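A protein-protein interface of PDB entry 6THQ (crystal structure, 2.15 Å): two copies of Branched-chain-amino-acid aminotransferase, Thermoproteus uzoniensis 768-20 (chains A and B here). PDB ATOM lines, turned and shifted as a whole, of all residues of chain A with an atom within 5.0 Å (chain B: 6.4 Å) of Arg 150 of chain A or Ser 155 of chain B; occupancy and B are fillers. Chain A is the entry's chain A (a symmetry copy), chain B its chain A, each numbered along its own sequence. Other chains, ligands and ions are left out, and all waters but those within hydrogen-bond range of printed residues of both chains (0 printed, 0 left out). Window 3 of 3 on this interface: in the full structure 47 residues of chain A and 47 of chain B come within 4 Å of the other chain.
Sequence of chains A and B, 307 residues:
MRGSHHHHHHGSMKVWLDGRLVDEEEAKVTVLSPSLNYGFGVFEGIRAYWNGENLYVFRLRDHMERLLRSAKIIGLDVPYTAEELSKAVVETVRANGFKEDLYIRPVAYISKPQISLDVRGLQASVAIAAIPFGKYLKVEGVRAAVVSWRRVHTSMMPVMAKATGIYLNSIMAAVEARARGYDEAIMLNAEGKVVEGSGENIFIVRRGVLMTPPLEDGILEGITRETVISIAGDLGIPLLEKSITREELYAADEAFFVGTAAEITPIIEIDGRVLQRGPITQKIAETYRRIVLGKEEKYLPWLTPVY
The side-chain hydroxyl (OG) of Ser 155 of chain B is in hydrogen-bond range of a ring nitrogen (ND1) of His 153 of chain B, at 2.8 Å. The backbone carbonyl oxygen (O) of Arg 150 of chain A is in hydrogen-bond range of the side-chain amide nitrogen (ND2) of Asn 169 of chain A, 2.9 Å away. The guanidinium group (NH1) of Arg 151 of chain A is in hydrogen-bond range of the side-chain amide oxygen (OD1) of Asn 169 of chain A, 3.0 Å away. The backbone carbonyl oxygen of Leu 188 of chain A lies within hydrogen-bond range of the backbone NH of Arg 151 of chain A (2.8 Å). The backbone NH (N) of Val 152 of chain A is in hydrogen-bond range of the side-chain amide oxygen (OD1) of Asn 169 of chain A, 3.0 Å away.
No position is printed for both chains.
Of the printed residues of chain B, Arg 150 of chain A touches Ser 155 (3.0 Å) and Met 156 (3.5 Å). Printed residues of chain A within 4 Å of Ser 155 of chain B: Trp 149 (3.7 Å) and Arg 150 (3.0 Å). Printed residues of chain B within 4 Å of Val 152 of chain A: Met 156 (3.8 Å). Of the printed residues of chain B, Asn 169 of chain A touches Met 156 (2.9 Å) and Met 157 (3.3 Å). The nearest printed residue of chain A that does not touch Ser 155 of chain B is Ser 148 of chain A (4.3 Å).
Thr 154 of chain B touches Trp 149 of chain A. O of Ser 155 of chain B touches CE3 of Trp 149 of chain A, at 3.7 Å. Met 156 of chain B touches Trp 149 of chain A. CZ3 of Trp 149 of chain A touches N of Met 157 of chain B (3.9 Å). Arg 150 of chain A touches Met 156 of chain B. Met 156 of chain B touches Arg 151 of chain A (CG to O, 3.7 Å). Val 152 of chain A touches Met 156 of chain B. Asn 169 of chain A touches Met 157 of chain B (N to CE, 3.3 Å).
Of the 11 printed residues of chain A, 5 touch a printed residue of chain B. Of the 5 printed residues of chain B, 4 touch a printed residue of chain A.
O of Ser 155 of chain B sits at hydrogen-bond distance from N of Arg 150 of chain A, at 3.0 Å. The backbone carbonyl oxygen of Met 156 of chain B lies within hydrogen-bond range of the side-chain amide nitrogen of Asn 169 of chain A, at 2.9 Å.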
ATOM      1  N   VAL A 147      20.396  13.075  18.962  1.00  0.00           N
ATOM      2  CA  VAL A 147      20.039  11.817  18.356  1.00  0.00           C
ATOM      3  C   VAL A 147      20.974  11.406  17.237  1.00  0.00           C
ATOM      4  O   VAL A 147      21.757  12.220  16.760  1.00  0.00           O
ATOM      5  CB  VAL A 147      18.569  11.794  17.869  1.00  0.00           C
ATOM      6  CG1 VAL A 147      17.631  11.855  19.076  1.00  0.00           C
ATOM      7  CG2 VAL A 147      18.248  12.894  16.899  1.00  0.00           C
ATOM      8  N   SER A 148      20.918  10.134  16.824  1.00  0.00           N
ATOM      9  CA  SER A 148      21.747   9.628  15.716  1.00  0.00           C
ATOM     10  C   SER A 148      21.304  10.158  14.322  1.00  0.00           C
ATOM     11  O   SER A 148      22.116  10.234  13.394  1.00  0.00           O
ATOM     12  CB  SER A 148      21.700   8.109  15.717  1.00  0.00           C
ATOM     13  OG  SER A 148      20.386   7.658  15.471  1.00  0.00           O
ATOM     14  N   TRP A 149      20.020  10.491  14.188  1.00  0.00           N
ATOM     15  CA  TRP A 149      19.473  10.991  12.922  1.00  0.00           C
ATOM     16  C   TRP A 149      19.898  12.430  12.720  1.00  0.00           C
ATOM     17  O   TRP A 149      19.668  13.260  13.605  1.00  0.00           O
ATOM     18  CB  TRP A 149      17.922  10.920  12.924  1.00  0.00           C
ATOM     19  CG  TRP A 149      17.432   9.546  12.889  1.00  0.00           C
ATOM     20  CD1 TRP A 149      16.986   8.786  13.992  1.00  0.00           C
ATOM     21  CD2 TRP A 149      17.384   8.667  11.743  1.00  0.00           C
ATOM     22  NE1 TRP A 149      16.650   7.537  13.560  1.00  0.00           N
ATOM     23  CE2 TRP A 149      16.860   7.422  12.200  1.00  0.00           C
ATOM     24  CE3 TRP A 149      17.670   8.823  10.387  1.00  0.00           C
ATOM     25  CZ2 TRP A 149      16.654   6.312  11.327  1.00  0.00           C
ATOM     26  CZ3 TRP A 149      17.429   7.734   9.501  1.00  0.00           C
ATOM     27  CH2 TRP A 149      16.953   6.496   9.991  1.00  0.00           C
ATOM     28  N   ARG A 150      20.428  12.729  11.545  1.00  0.00           N
ATOM     29  CA  ARG A 150      20.767  14.088  11.165  1.00  0.00           C
ATOM     30  C   ARG A 150      19.571  14.797  10.582  1.00  0.00           C
ATOM     31  O   ARG A 150      18.687  14.154   9.996  1.00  0.00           O
ATOM     32  CB  ARG A 150      21.939  14.096  10.157  1.00  0.00           C
ATOM     33  CG  ARG A 150      23.308  13.589  10.711  1.00  0.00           C
ATOM     34  CD  ARG A 150      23.841  14.434  11.912  1.00  0.00           C
ATOM     35  NE  ARG A 150      25.157  14.056  12.436  1.00  0.00           N
ATOM     36  CZ  ARG A 150      25.389  13.289  13.519  1.00  0.00           C
ATOM     37  NH1 ARG A 150      24.397  12.778  14.197  1.00  0.00           N
ATOM     38  NH2 ARG A 150      26.647  13.042  13.938  1.00  0.00           N
ATOM     39  N   ARG A 151      19.492  16.120  10.798  1.00  0.00           N
ATOM     40  CA  ARG A 151      18.440  16.863  10.171  1.00  0.00           C
ATOM     41  C   ARG A 151      18.563  16.778   8.647  1.00  0.00           C
ATOM     42  O   ARG A 151      19.678  16.953   8.108  1.00  0.00           O
ATOM     43  CB  ARG A 151      18.573  18.343  10.557  1.00  0.00           C
ATOM     44  CG  ARG A 151      17.359  19.164  10.103  1.00  0.00           C
ATOM     45  CD  ARG A 151      16.176  18.831  11.006  1.00  0.00           C
ATOM     46  NE  ARG A 151      15.166  19.844  10.884  1.00  0.00           N
ATOM     47  CZ  ARG A 151      13.966  19.642  10.335  1.00  0.00           C
ATOM     48  NH1 ARG A 151      13.643  18.434   9.915  1.00  0.00           N
ATOM     49  NH2 ARG A 151      13.080  20.639  10.242  1.00  0.00           N
ATOM     50  N   VAL A 152      17.444  16.670   7.937  1.00  0.00           N
ATOM     51  CA  VAL A 152      17.554  16.546   6.494  1.00  0.00           C
ATOM     52  C   VAL A 152      18.139  17.788   5.914  1.00  0.00           C
ATOM     53  O   VAL A 152      17.835  18.924   6.352  1.00  0.00           O
ATOM     54  CB  VAL A 152      16.192  16.508   5.727  1.00  0.00           C
ATOM     55  CG1 VAL A 152      15.925  15.246   5.036  1.00  0.00           C
ATOM     56  CG2 VAL A 152      15.037  17.033   6.458  1.00  0.00           C
ATOM     57  N   ASN A 169      11.666  12.718   9.022  1.00  0.00           N
ATOM     58  CA  ASN A 169      12.931  13.044   9.689  1.00  0.00           C
ATOM     59  C   ASN A 169      12.676  13.431  11.172  1.00  0.00           C
ATOM     60  O   ASN A 169      13.385  12.931  12.056  1.00  0.00           O
ATOM     61  CB  ASN A 169      13.584  14.194   8.920  1.00  0.00           C
ATOM     62  CG  ASN A 169      14.939  14.633   9.462  1.00  0.00           C
ATOM     63  OD1 ASN A 169      15.154  15.835   9.677  1.00  0.00           O
ATOM     64  ND2 ASN A 169      15.904  13.693   9.581  1.00  0.00           N
ATOM     65  N   MET A 187      18.671  17.557  17.030  1.00  0.00           N
ATOM     66  CA  MET A 187      19.357  17.148  15.815  1.00  0.00           C
ATOM     67  C   MET A 187      20.503  18.010  15.392  1.00  0.00           C
ATOM     68  O   MET A 187      20.433  19.256  15.461  1.00  0.00           O
ATOM     69  CB  MET A 187      18.359  17.141  14.664  1.00  0.00           C
ATOM     70  CG  MET A 187      17.434  15.955  14.763  1.00  0.00           C
ATOM     71  SD  MET A 187      16.407  15.644  13.311  1.00  0.00           S
ATOM     72  CE  MET A 187      15.195  16.804  13.871  1.00  0.00           C
ATOM     73  N   LEU A 188      21.537  17.341  14.892  1.00  0.00           N
ATOM     74  CA  LEU A 188      22.648  18.043  14.217  1.00  0.00           C
ATOM     75  C   LEU A 188      22.364  18.105  12.748  1.00  0.00           C
ATOM     76  O   LEU A 188      21.666  17.238  12.220  1.00  0.00           O
ATOM     77  CB  LEU A 188      24.005  17.361  14.461  1.00  0.00           C
ATOM     78  CG  LEU A 188      24.328  17.002  15.913  1.00  0.00           C
ATOM     79  CD1 LEU A 188      25.678  16.279  16.032  1.00  0.00           C
ATOM     80  CD2 LEU A 188      24.280  18.264  16.799  1.00  0.00           C
ATOM     81  N   ASN A 189      22.888  19.124  12.070  1.00  0.00           N
ATOM     82  CA  ASN A 189      22.856  19.118  10.619  1.00  0.00           C
ATOM     83  C   ASN A 189      23.994  18.316   9.987  1.00  0.00           C
ATOM     84  O   ASN A 189      24.868  17.730  10.683  1.00  0.00           O
ATOM     85  CB  ASN A 189      22.749  20.524  10.043  1.00  0.00           C
ATOM     86  CG  ASN A 189      24.032  21.341  10.195  1.00  0.00           C
ATOM     87  OD1 ASN A 189      25.081  20.819  10.620  1.00  0.00           O
ATOM     88  ND2 ASN A 189      23.939  22.705   9.881  1.00  0.00           N
ATOM     89  N   ALA A 190      24.024  18.316   8.649  1.00  0.00           N
ATOM     90  CA  ALA A 190      25.037  17.518   7.935  1.00  0.00           C
ATOM     91  C   ALA A 190      26.428  17.925   8.314  1.00  0.00           C
ATOM     92  O   ALA A 190      27.293  17.147   8.191  1.00  0.00           O
ATOM     93  CB  ALA A 190      24.851  17.670   6.449  1.00  0.00           C
ATOM     94  N   HIS B 153      19.619  11.342   1.936  1.00  0.00           N
ATOM     95  CA  HIS B 153      20.710  10.517   2.450  1.00  0.00           C
ATOM     96  C   HIS B 153      20.287   9.689   3.635  1.00  0.00           C
ATOM     97  O   HIS B 153      19.484  10.116   4.480  1.00  0.00           O
ATOM     98  CB  HIS B 153      21.838  11.445   2.888  1.00  0.00           C
ATOM     99  CG  HIS B 153      23.130  10.742   3.158  1.00  0.00           C
ATOM    100  ND1 HIS B 153      23.549  10.415   4.427  1.00  0.00           N
ATOM    101  CD2 HIS B 153      24.094  10.299   2.314  1.00  0.00           C
ATOM    102  CE1 HIS B 153      24.729   9.825   4.353  1.00  0.00           C
ATOM    103  NE2 HIS B 153      25.087   9.763   3.081  1.00  0.00           N
ATOM    104  N   THR B 154      20.916   8.526   3.730  1.00  0.00           N
ATOM    105  CA  THR B 154      20.596   7.492   4.724  1.00  0.00           C
ATOM    106  C   THR B 154      20.739   8.008   6.179  1.00  0.00           C
ATOM    107  O   THR B 154      20.039   7.556   7.134  1.00  0.00           O
ATOM    108  CB  THR B 154      21.470   6.224   4.492  1.00  0.00           C
ATOM    109  OG1 THR B 154      21.140   5.251   5.463  1.00  0.00           O
ATOM    110  CG2 THR B 154      23.042   6.526   4.586  1.00  0.00           C
ATOM    111  N   SER B 155      21.650   8.960   6.380  1.00  0.00           N
ATOM    112  CA  SER B 155      21.888   9.459   7.747  1.00  0.00           C
ATOM    113  C   SER B 155      20.756  10.364   8.203  1.00  0.00           C
ATOM    114  O   SER B 155      20.700  10.736   9.374  1.00  0.00           O
ATOM    115  CB  SER B 155      23.180  10.269   7.774  1.00  0.00           C
ATOM    116  OG  SER B 155      22.978  11.435   6.949  1.00  0.00           O
ATOM    117  N   MET B 156      19.884  10.730   7.263  1.00  0.00           N
ATOM    118  CA  MET B 156      18.732  11.624   7.520  1.00  0.00           C
ATOM    119  C   MET B 156      17.367  10.964   7.386  1.00  0.00           C
ATOM    120  O   MET B 156      16.481  11.271   8.126  1.00  0.00           O
ATOM    121  CB  MET B 156      18.752  12.752   6.541  1.00  0.00           C
ATOM    122  CG  MET B 156      20.013  13.564   6.645  1.00  0.00           C
ATOM    123  SD  MET B 156      20.347  14.454   5.105  1.00  0.00           S
ATOM    124  CE  MET B 156      22.010  14.927   5.590  1.00  0.00           C
ATOM    125  N   MET B 157      17.199  10.104   6.390  1.00  0.00           N
ATOM    126  CA  MET B 157      15.940   9.413   6.199  1.00  0.00           C
ATOM    127  C   MET B 157      16.260   8.028   5.679  1.00  0.00           C
ATOM    128  O   MET B 157      17.256   7.837   5.080  1.00  0.00           O
ATOM    129  CB  MET B 157      15.027  10.158   5.221  1.00  0.00           C
ATOM    130  CG  MET B 157      14.300  11.295   5.930  1.00  0.00           C
ATOM    131  SD  MET B 157      13.235  12.063   4.736  1.00  0.00           S
ATOM    132  CE  MET B 157      12.231  13.051   5.790  1.00  0.00           C
